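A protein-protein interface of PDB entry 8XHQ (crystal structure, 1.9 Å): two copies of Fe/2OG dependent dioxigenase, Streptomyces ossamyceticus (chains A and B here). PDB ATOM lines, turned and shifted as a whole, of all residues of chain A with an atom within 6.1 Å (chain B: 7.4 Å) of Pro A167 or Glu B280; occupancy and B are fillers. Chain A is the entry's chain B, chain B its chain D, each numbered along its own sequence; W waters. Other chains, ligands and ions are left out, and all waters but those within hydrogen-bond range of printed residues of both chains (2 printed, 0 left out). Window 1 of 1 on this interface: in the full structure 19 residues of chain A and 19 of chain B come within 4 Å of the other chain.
Water W1 lies within hydrogen-bond range of the backbone carbonyl oxygen of Pro A167 and the backbone carbonyl oxygen of Glu B280.
Water W2 bridges the indole nitrogen of Trp A192 and the side-chain amide oxygen of Asn B279.
Pro A167 touches Glu B280, and with the chains exchanged Glu A280 touches Pro B167.
Positions printed for both chains: 86, 166, 167, 280 and 281.
Leu A163 touches Ser B283 (CD1 to OG, 3.9 Å).
Pro A167 touches Asn B279 (CG to O, 3.8 Å).
Glu B280 touches Pro A167 (O to CG, 3.4 Å).
Pro A167 touches Ser B283.
OG of Ser B283 touches NE1 of Trp A192, at 3.9 Å.
Leu A225 touches Asp B276.
Leu A225 touches Glu B280.
Glu A280 touches Pro B167 (O to CG, 3.6 Å).
Pro A167 touches just these residues of chain B: Asn B279 (3.8 Å), Glu B280 (3.4 Å) and Ser B283 (3.9 Å).
Of chain A, only Pro A167 (3.4 Å) and Leu A225 (3.8 Å) come within 4 Å of Glu B280.
Printed residues of chain B within 4 Å of Glu A280: Pro B167.
Printed residues of chain A within 4 Å of Ser B283: Leu A163 (3.9 Å), Pro A167 (3.9 Å), Trp A192 (3.9 Å) and Arg A227 (2.7 Å).
Of the printed residues of chain B, Leu A225 touches Asp B276 (3.998 Å) and Glu B280 (3.8 Å).
Of the printed residues of chain A, Asp B276 touches Leu A225 (3.998 Å).
The nearest residue of chain B that does not touch Pro A167 is Thr B281 (5.2 Å).
The nearest printed residue of chain A that does not touch Ser B283 is Cys A165 (6.5 Å).
The backbone carbonyl oxygen (O) of Asn B279 is in hydrogen-bond range of the side-chain hydroxyl (OG) of Ser B283 (3.0 Å).
The backbone carbonyl oxygen (O) of Asn B278 lies within hydrogen-bond range of the backbone NH (N) of Ser B283 (2.9 Å).
Printed residues of chain A that touch a printed residue of chain B: Leu A163, Pro A167, Trp A192, Leu A225, Arg A227 and Glu A280.
Among the printed residues, no Asp or Glu carboxylate lies within 4 Å of a Lys or Arg side-chain nitrogen of the other chain.
NE1 of Trp A192 is in hydrogen-bond range of OD1 of Asn B279, 3.5 Å away.
The guanidinium group of Arg A227 sits at hydrogen-bond distance from the side-chain hydroxyl of Ser B283 (2.7 Å).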
ATOM      1  N   TYR A  86      17.515  -9.925  30.965  1.00  0.00           N
ATOM      2  CA  TYR A  86      17.400  -8.908  29.929  1.00  0.00           C
ATOM      3  C   TYR A  86      16.204  -8.011  30.198  1.00  0.00           C
ATOM      4  O   TYR A  86      15.292  -8.365  30.944  1.00  0.00           O
ATOM      5  CB  TYR A  86      17.287  -9.559  28.547  1.00  0.00           C
ATOM      6  CG  TYR A  86      18.511 -10.396  28.259  1.00  0.00           C
ATOM      7  CD1 TYR A  86      19.684  -9.805  27.821  1.00  0.00           C
ATOM      8  CD2 TYR A  86      18.496 -11.774  28.457  1.00  0.00           C
ATOM      9  CE1 TYR A  86      20.821 -10.570  27.562  1.00  0.00           C
ATOM     10  CE2 TYR A  86      19.614 -12.543  28.201  1.00  0.00           C
ATOM     11  CZ  TYR A  86      20.775 -11.935  27.759  1.00  0.00           C
ATOM     12  OH  TYR A  86      21.885 -12.707  27.509  1.00  0.00           O
ATOM     13  N   LEU A 163      21.140  -5.408  29.172  1.00  0.00           N
ATOM     14  CA  LEU A 163      20.916  -5.447  27.728  1.00  0.00           C
ATOM     15  C   LEU A 163      19.433  -5.596  27.424  1.00  0.00           C
ATOM     16  O   LEU A 163      18.690  -6.237  28.169  1.00  0.00           O
ATOM     17  CB  LEU A 163      21.656  -6.617  27.077  1.00  0.00           C
ATOM     18  CG  LEU A 163      23.070  -6.430  26.521  1.00  0.00           C
ATOM     19  CD1 LEU A 163      23.439  -7.661  25.706  1.00  0.00           C
ATOM     20  CD2 LEU A 163      23.174  -5.192  25.641  1.00  0.00           C
ATOM     21  N   CYS A 165      17.856  -7.165  24.594  1.00  0.00           N
ATOM     22  CA  CYS A 165      17.545  -8.515  24.122  1.00  0.00           C
ATOM     23  C   CYS A 165      18.842  -9.293  23.983  1.00  0.00           C
ATOM     24  O   CYS A 165      19.821  -8.758  23.459  1.00  0.00           O
ATOM     25  CB  CYS A 165      16.828  -8.480  22.749  1.00  0.00           C
ATOM     26  SG  CYS A 165      16.190 -10.049  22.138  1.00  0.00           S
ATOM     27  N   ALA A 166      18.846 -10.555  24.422  1.00  0.00           N
ATOM     28  CA  ALA A 166      20.023 -11.396  24.220  1.00  0.00           C
ATOM     29  C   ALA A 166      20.450 -11.370  22.758  1.00  0.00           C
ATOM     30  O   ALA A 166      19.597 -11.370  21.855  1.00  0.00           O
ATOM     31  CB  ALA A 166      19.751 -12.845  24.626  1.00  0.00           C
ATOM     32  N   PRO A 167      21.748 -11.340  22.484  1.00  0.00           N
ATOM     33  CA  PRO A 167      22.204 -11.537  21.103  1.00  0.00           C
ATOM     34  C   PRO A 167      21.788 -12.921  20.622  1.00  0.00           C
ATOM     35  O   PRO A 167      21.943 -13.911  21.335  1.00  0.00           O
ATOM     36  CB  PRO A 167      23.727 -11.385  21.193  1.00  0.00           C
ATOM     37  CG  PRO A 167      24.054 -11.486  22.649  1.00  0.00           C
ATOM     38  CD  PRO A 167      22.847 -11.062  23.422  1.00  0.00           C
ATOM     39  N   HIS A 168      21.203 -12.981  19.426  1.00  0.00           N
ATOM     40  CA  HIS A 168      20.762 -14.275  18.925  1.00  0.00           C
ATOM     41  C   HIS A 168      20.663 -14.245  17.411  1.00  0.00           C
ATOM     42  O   HIS A 168      20.612 -13.181  16.783  1.00  0.00           O
ATOM     43  CB  HIS A 168      19.403 -14.682  19.507  1.00  0.00           C
ATOM     44  CG  HIS A 168      18.299 -13.726  19.174  1.00  0.00           C
ATOM     45  ND1 HIS A 168      18.128 -12.530  19.839  1.00  0.00           N
ATOM     46  CD2 HIS A 168      17.315 -13.782  18.242  1.00  0.00           C
ATOM     47  CE1 HIS A 168      17.090 -11.890  19.335  1.00  0.00           C
ATOM     48  NE2 HIS A 168      16.574 -12.636  18.374  1.00  0.00           N
ATOM     49  N   LYS A 169      20.636 -15.443  16.841  1.00  0.00           N
ATOM     50  CA  LYS A 169      20.090 -15.674  15.514  1.00  0.00           C
ATOM     51  C   LYS A 169      18.681 -16.222  15.665  1.00  0.00           C
ATOM     52  O   LYS A 169      18.447 -17.120  16.476  1.00  0.00           O
ATOM     53  CB  LYS A 169      20.951 -16.656  14.710  1.00  0.00           C
ATOM     54  CG  LYS A 169      22.423 -16.202  14.539  1.00  0.00           C
ATOM     55  CD  LYS A 169      23.219 -17.261  13.713  1.00  0.00           C
ATOM     56  CE  LYS A 169      24.675 -16.834  13.476  1.00  0.00           C
ATOM     57  NZ  LYS A 169      25.409 -17.858  12.631  1.00  0.00           N
ATOM     58  N   TRP A 192      29.032  -4.353  15.766  1.00  0.00           N
ATOM     59  CA  TRP A 192      27.605  -4.089  15.924  1.00  0.00           C
ATOM     60  C   TRP A 192      27.205  -2.871  15.091  1.00  0.00           C
ATOM     61  O   TRP A 192      27.679  -1.757  15.342  1.00  0.00           O
ATOM     62  CB  TRP A 192      27.259  -3.863  17.397  1.00  0.00           C
ATOM     63  CG  TRP A 192      27.216  -5.121  18.250  1.00  0.00           C
ATOM     64  CD1 TRP A 192      27.995  -5.405  19.343  1.00  0.00           C
ATOM     65  CD2 TRP A 192      26.345  -6.248  18.074  1.00  0.00           C
ATOM     66  NE1 TRP A 192      27.660  -6.644  19.854  1.00  0.00           N
ATOM     67  CE2 TRP A 192      26.651  -7.179  19.093  1.00  0.00           C
ATOM     68  CE3 TRP A 192      25.337  -6.559  17.153  1.00  0.00           C
ATOM     69  CZ2 TRP A 192      25.979  -8.397  19.221  1.00  0.00           C
ATOM     70  CZ3 TRP A 192      24.674  -7.770  17.277  1.00  0.00           C
ATOM     71  CH2 TRP A 192      25.003  -8.682  18.297  1.00  0.00           C
ATOM     72  N   LEU A 225      23.103 -12.194  13.122  1.00  0.00           N
ATOM     73  CA  LEU A 225      23.260 -12.142  14.564  1.00  0.00           C
ATOM     74  C   LEU A 225      22.870 -10.749  15.015  1.00  0.00           C
ATOM     75  O   LEU A 225      23.421  -9.763  14.515  1.00  0.00           O
ATOM     76  CB  LEU A 225      24.713 -12.452  14.940  1.00  0.00           C
ATOM     77  CG  LEU A 225      25.041 -12.278  16.422  1.00  0.00           C
ATOM     78  CD1 LEU A 225      24.230 -13.275  17.246  1.00  0.00           C
ATOM     79  CD2 LEU A 225      26.542 -12.415  16.675  1.00  0.00           C
ATOM     80  N   HIS A 226      21.905 -10.652  15.923  1.00  0.00           N
ATOM     81  CA  HIS A 226      21.378  -9.344  16.269  1.00  0.00           C
ATOM     82  C   HIS A 226      21.013  -9.304  17.741  1.00  0.00           C
ATOM     83  O   HIS A 226      20.764 -10.333  18.374  1.00  0.00           O
ATOM     84  CB  HIS A 226      20.166  -8.987  15.390  1.00  0.00           C
ATOM     85  CG  HIS A 226      19.083 -10.019  15.399  1.00  0.00           C
ATOM     86  ND1 HIS A 226      19.180 -11.208  14.712  1.00  0.00           N
ATOM     87  CD2 HIS A 226      17.866 -10.023  15.988  1.00  0.00           C
ATOM     88  CE1 HIS A 226      18.080 -11.912  14.894  1.00  0.00           C
ATOM     89  NE2 HIS A 226      17.257 -11.205  15.647  1.00  0.00           N
ATOM     90  N   ARG A 227      21.000  -8.089  18.284  1.00  0.00           N
ATOM     91  CA  ARG A 227      20.613  -7.868  19.666  1.00  0.00           C
ATOM     92  C   ARG A 227      19.843  -6.558  19.741  1.00  0.00           C
ATOM     93  O   ARG A 227      19.800  -5.788  18.781  1.00  0.00           O
ATOM     94  CB  ARG A 227      21.839  -7.804  20.588  1.00  0.00           C
ATOM     95  CG  ARG A 227      22.755  -6.629  20.286  1.00  0.00           C
ATOM     96  CD  ARG A 227      23.893  -6.489  21.317  1.00  0.00           C
ATOM     97  NE  ARG A 227      24.523  -5.179  21.209  1.00  0.00           N
ATOM     98  CZ  ARG A 227      25.546  -4.765  21.953  1.00  0.00           C
ATOM     99  NH1 ARG A 227      26.034  -3.538  21.784  1.00  0.00           N
ATOM    100  NH2 ARG A 227      26.081  -5.572  22.867  1.00  0.00           N
ATOM    101  N   VAL A 228      19.269  -6.291  20.911  1.00  0.00           N
ATOM    102  CA  VAL A 228      18.777  -4.958  21.251  1.00  0.00           C
ATOM    103  C   VAL A 228      19.619  -4.425  22.407  1.00  0.00           C
ATOM    104  O   VAL A 228      19.669  -5.038  23.478  1.00  0.00           O
ATOM    105  CB  VAL A 228      17.283  -4.970  21.603  1.00  0.00           C
ATOM    106  CG1 VAL A 228      16.820  -3.562  21.933  1.00  0.00           C
ATOM    107  CG2 VAL A 228      16.477  -5.512  20.409  1.00  0.00           C
ATOM    108  N   GLU A 280      22.169 -21.435  25.068  1.00  0.00           N
ATOM    109  CA  GLU A 280      23.226 -20.457  24.856  1.00  0.00           C
ATOM    110  C   GLU A 280      22.716 -19.022  24.765  1.00  0.00           C
ATOM    111  O   GLU A 280      23.496 -18.094  24.979  1.00  0.00           O
ATOM    112  CB  GLU A 280      24.039 -20.787  23.601  1.00  0.00           C
ATOM    113  CG  GLU A 280      23.302 -20.628  22.291  1.00  0.00           C
ATOM    114  CD  GLU A 280      24.128 -21.110  21.115  1.00  0.00           C
ATOM    115  OE1 GLU A 280      23.538 -21.443  20.062  1.00  0.00           O
ATOM    116  OE2 GLU A 280      25.371 -21.166  21.253  1.00  0.00           O
ATOM    117  N   THR A 281      21.434 -18.817  24.480  1.00  0.00           N
ATOM    118  CA  THR A 281      20.898 -17.479  24.250  1.00  0.00           C
ATOM    119  C   THR A 281      20.319 -16.890  25.530  1.00  0.00           C
ATOM    120  O   THR A 281      20.690 -15.787  25.951  1.00  0.00           O
ATOM    121  CB  THR A 281      19.802 -17.520  23.170  1.00  0.00           C
ATOM    122  OG1 THR A 281      20.320 -18.061  21.956  1.00  0.00           O
ATOM    123  CG2 THR A 281      19.256 -16.120  22.911  1.00  0.00           C
ATOM    124  N   TYR B  86      28.103 -10.556  34.058  1.00  0.00           N
ATOM    125  CA  TYR B  86      28.437 -11.876  34.599  1.00  0.00           C
ATOM    126  C   TYR B  86      29.305 -11.762  35.845  1.00  0.00           C
ATOM    127  O   TYR B  86      30.103 -10.831  35.987  1.00  0.00           O
ATOM    128  CB  TYR B  86      29.159 -12.756  33.564  1.00  0.00           C
ATOM    129  CG  TYR B  86      28.294 -13.012  32.360  1.00  0.00           C
ATOM    130  CD1 TYR B  86      27.301 -13.978  32.388  1.00  0.00           C
ATOM    131  CD2 TYR B  86      28.436 -12.252  31.214  1.00  0.00           C
ATOM    132  CE1 TYR B  86      26.480 -14.186  31.298  1.00  0.00           C
ATOM    133  CE2 TYR B  86      27.623 -12.457  30.121  1.00  0.00           C
ATOM    134  CZ  TYR B  86      26.645 -13.422  30.171  1.00  0.00           C
ATOM    135  OH  TYR B  86      25.847 -13.630  29.071  1.00  0.00           O
ATOM    136  N   ALA B 166      29.197 -16.648  31.054  1.00  0.00           N
ATOM    137  CA  ALA B 166      28.359 -16.721  29.864  1.00  0.00           C
ATOM    138  C   ALA B 166      28.432 -18.118  29.259  1.00  0.00           C
ATOM    139  O   ALA B 166      29.507 -18.728  29.230  1.00  0.00           O
ATOM    140  CB  ALA B 166      28.790 -15.699  28.813  1.00  0.00           C
ATOM    141  N   PRO B 167      27.313 -18.658  28.783  1.00  0.00           N
ATOM    142  CA  PRO B 167      27.375 -19.909  28.025  1.00  0.00           C
ATOM    143  C   PRO B 167      28.184 -19.700  26.757  1.00  0.00           C
ATOM    144  O   PRO B 167      28.014 -18.706  26.049  1.00  0.00           O
ATOM    145  CB  PRO B 167      25.907 -20.245  27.730  1.00  0.00           C
ATOM    146  CG  PRO B 167      25.109 -19.032  28.112  1.00  0.00           C
ATOM    147  CD  PRO B 167      25.947 -18.146  28.978  1.00  0.00           C
ATOM    148  N   PHE B 273      35.806 -14.562  13.089  1.00  0.00           N
ATOM    149  CA  PHE B 273      35.205 -15.593  13.930  1.00  0.00           C
ATOM    150  C   PHE B 273      35.208 -15.168  15.390  1.00  0.00           C
ATOM    151  O   PHE B 273      34.206 -15.317  16.096  1.00  0.00           O
ATOM    152  CB  PHE B 273      35.952 -16.918  13.761  1.00  0.00           C
ATOM    153  CG  PHE B 273      35.490 -18.007  14.699  1.00  0.00           C
ATOM    154  CD1 PHE B 273      36.108 -18.202  15.927  1.00  0.00           C
ATOM    155  CD2 PHE B 273      34.434 -18.836  14.353  1.00  0.00           C
ATOM    156  CE1 PHE B 273      35.683 -19.203  16.787  1.00  0.00           C
ATOM    157  CE2 PHE B 273      34.006 -19.839  15.212  1.00  0.00           C
ATOM    158  CZ  PHE B 273      34.628 -20.023  16.428  1.00  0.00           C
ATOM    159  N   LEU B 274      36.339 -14.648  15.865  1.00  0.00           N
ATOM    160  CA  LEU B 274      36.441 -14.265  17.266  1.00  0.00           C
ATOM    161  C   LEU B 274      35.564 -13.063  17.583  1.00  0.00           C
ATOM    162  O   LEU B 274      34.998 -12.975  18.679  1.00  0.00           O
ATOM    163  CB  LEU B 274      37.898 -13.974  17.623  1.00  0.00           C
ATOM    164  CG  LEU B 274      38.793 -15.212  17.670  1.00  0.00           C
ATOM    165  CD1 LEU B 274      40.236 -14.807  17.962  1.00  0.00           C
ATOM    166  CD2 LEU B 274      38.263 -16.182  18.710  1.00  0.00           C
ATOM    167  N   ARG B 275      35.455 -12.114  16.653  1.00  0.00           N
ATOM    168  CA  ARG B 275      34.627 -10.944  16.911  1.00  0.00           C
ATOM    169  C   ARG B 275      33.160 -11.328  17.024  1.00  0.00           C
ATOM    170  O   ARG B 275      32.458 -10.839  17.910  1.00  0.00           O
ATOM    171  CB  ARG B 275      34.836  -9.893  15.821  1.00  0.00           C
ATOM    172  CG  ARG B 275      36.237  -9.313  15.840  1.00  0.00           C
ATOM    173  CD  ARG B 275      36.355  -8.033  15.045  1.00  0.00           C
ATOM    174  NE  ARG B 275      37.707  -7.506  15.171  1.00  0.00           N
ATOM    175  CZ  ARG B 275      38.155  -6.846  16.236  1.00  0.00           C
ATOM    176  NH1 ARG B 275      37.350  -6.621  17.265  1.00  0.00           N
ATOM    177  NH2 ARG B 275      39.407  -6.409  16.272  1.00  0.00           N
ATOM    178  N   ASP B 276      32.693 -12.223  16.151  1.00  0.00           N
ATOM    179  CA  ASP B 276      31.331 -12.743  16.267  1.00  0.00           C
ATOM    180  C   ASP B 276      31.125 -13.453  17.595  1.00  0.00           C
ATOM    181  O   ASP B 276      30.113 -13.230  18.278  1.00  0.00           O
ATOM    182  CB  ASP B 276      31.030 -13.699  15.115  1.00  0.00           C
ATOM    183  CG  ASP B 276      30.805 -12.980  13.804  1.00  0.00           C
ATOM    184  OD1 ASP B 276      30.420 -11.789  13.843  1.00  0.00           O
ATOM    185  OD2 ASP B 276      30.998 -13.615  12.744  1.00  0.00           O
ATOM    186  N   PHE B 277      32.072 -14.320  17.968  1.00  0.00           N
ATOM    187  CA  PHE B 277      32.041 -14.970  19.273  1.00  0.00           C
ATOM    188  C   PHE B 277      31.870 -13.956  20.397  1.00  0.00           C
ATOM    189  O   PHE B 277      31.004 -14.126  21.267  1.00  0.00           O
ATOM    190  CB  PHE B 277      33.317 -15.787  19.475  1.00  0.00           C
ATOM    191  CG  PHE B 277      33.488 -16.285  20.868  1.00  0.00           C
ATOM    192  CD1 PHE B 277      32.922 -17.484  21.255  1.00  0.00           C
ATOM    193  CD2 PHE B 277      34.210 -15.554  21.795  1.00  0.00           C
ATOM    194  CE1 PHE B 277      33.065 -17.937  22.538  1.00  0.00           C
ATOM    195  CE2 PHE B 277      34.359 -16.003  23.075  1.00  0.00           C
ATOM    196  CZ  PHE B 277      33.786 -17.198  23.451  1.00  0.00           C
ATOM    197  N   ASN B 278      32.707 -12.903  20.419  1.00  0.00           N
ATOM    198  CA  ASN B 278      32.641 -11.929  21.513  1.00  0.00           C
ATOM    199  C   ASN B 278      31.292 -11.226  21.541  1.00  0.00           C
ATOM    200  O   ASN B 278      30.704 -11.020  22.609  1.00  0.00           O
ATOM    201  CB  ASN B 278      33.762 -10.884  21.390  1.00  0.00           C
ATOM    202  CG  ASN B 278      35.142 -11.450  21.755  1.00  0.00           C
ATOM    203  OD1 ASN B 278      35.242 -12.512  22.363  1.00  0.00           O
ATOM    204  ND2 ASN B 278      36.196 -10.743  21.385  1.00  0.00           N
ATOM    205  N   ASN B 279      30.797 -10.855  20.363  1.00  0.00           N
ATOM    206  CA  ASN B 279      29.528 -10.154  20.255  1.00  0.00           C
ATOM    207  C   ASN B 279      28.373 -10.986  20.798  1.00  0.00           C
ATOM    208  O   ASN B 279      27.493 -10.453  21.491  1.00  0.00           O
ATOM    209  CB  ASN B 279      29.293  -9.776  18.792  1.00  0.00           C
ATOM    210  CG  ASN B 279      30.159  -8.621  18.357  1.00  0.00           C
ATOM    211  OD1 ASN B 279      30.812  -7.972  19.181  1.00  0.00           O
ATOM    212  ND2 ASN B 279      30.135  -8.321  17.070  1.00  0.00           N
ATOM    213  N   GLU B 280      28.340 -12.288  20.489  1.00  0.00           N
ATOM    214  CA  GLU B 280      27.230 -13.100  20.972  1.00  0.00           C
ATOM    215  C   GLU B 280      27.440 -13.672  22.368  1.00  0.00           C
ATOM    216  O   GLU B 280      26.449 -13.930  23.057  1.00  0.00           O
ATOM    217  CB  GLU B 280      26.921 -14.233  19.998  1.00  0.00           C
ATOM    218  CG  GLU B 280      27.923 -15.346  19.935  1.00  0.00           C
ATOM    219  CD  GLU B 280      27.619 -16.276  18.779  1.00  0.00           C
ATOM    220  OE1 GLU B 280      28.547 -16.952  18.278  1.00  0.00           O
ATOM    221  OE2 GLU B 280      26.443 -16.306  18.358  1.00  0.00           O
ATOM    222  N   THR B 281      28.690 -13.840  22.817  1.00  0.00           N
ATOM    223  CA  THR B 281      28.984 -14.435  24.123  1.00  0.00           C
ATOM    224  C   THR B 281      28.989 -13.389  25.233  1.00  0.00           C
ATOM    225  O   THR B 281      28.281 -13.522  26.235  1.00  0.00           O
ATOM    226  CB  THR B 281      30.345 -15.149  24.089  1.00  0.00           C
ATOM    227  OG1 THR B 281      30.349 -16.133  23.049  1.00  0.00           O
ATOM    228  CG2 THR B 281      30.649 -15.825  25.432  1.00  0.00           C
ATOM    229  N   TRP B 282      29.803 -12.356  25.073  1.00  0.00           N
ATOM    230  CA  TRP B 282      29.989 -11.355  26.112  1.00  0.00           C
ATOM    231  C   TRP B 282      29.216 -10.074  25.837  1.00  0.00           C
ATOM    232  O   TRP B 282      28.575  -9.542  26.742  1.00  0.00           O
ATOM    233  CB  TRP B 282      31.484 -11.065  26.268  1.00  0.00           C
ATOM    234  CG  TRP B 282      32.255 -12.330  26.666  1.00  0.00           C
ATOM    235  CD1 TRP B 282      33.117 -13.052  25.890  1.00  0.00           C
ATOM    236  CD2 TRP B 282      32.178 -13.019  27.923  1.00  0.00           C
ATOM    237  NE1 TRP B 282      33.592 -14.147  26.589  1.00  0.00           N
ATOM    238  CE2 TRP B 282      33.031 -14.147  27.839  1.00  0.00           C
ATOM    239  CE3 TRP B 282      31.481 -12.787  29.116  1.00  0.00           C
ATOM    240  CZ2 TRP B 282      33.210 -15.028  28.905  1.00  0.00           C
ATOM    241  CZ3 TRP B 282      31.648 -13.673  30.169  1.00  0.00           C
ATOM    242  CH2 TRP B 282      32.508 -14.782  30.055  1.00  0.00           C
ATOM    243  N   SER B 283      29.252  -9.583  24.600  1.00  0.00           N
ATOM    244  CA  SER B 283      28.429  -8.451  24.178  1.00  0.00           C
ATOM    245  C   SER B 283      28.687  -7.212  25.027  1.00  0.00           C
ATOM    246  O   SER B 283      27.763  -6.436  25.297  1.00  0.00           O
ATOM    247  CB  SER B 283      26.939  -8.820  24.209  1.00  0.00           C
ATOM    248  OG  SER B 283      26.262  -8.267  23.105  1.00  0.00           O
HETATM  249  O   HOH W   1      23.467 -14.481  23.541  1.00  0.00           O
HETATM  250  O   HOH W   2      29.825  -6.244  22.047  1.00  0.00           O
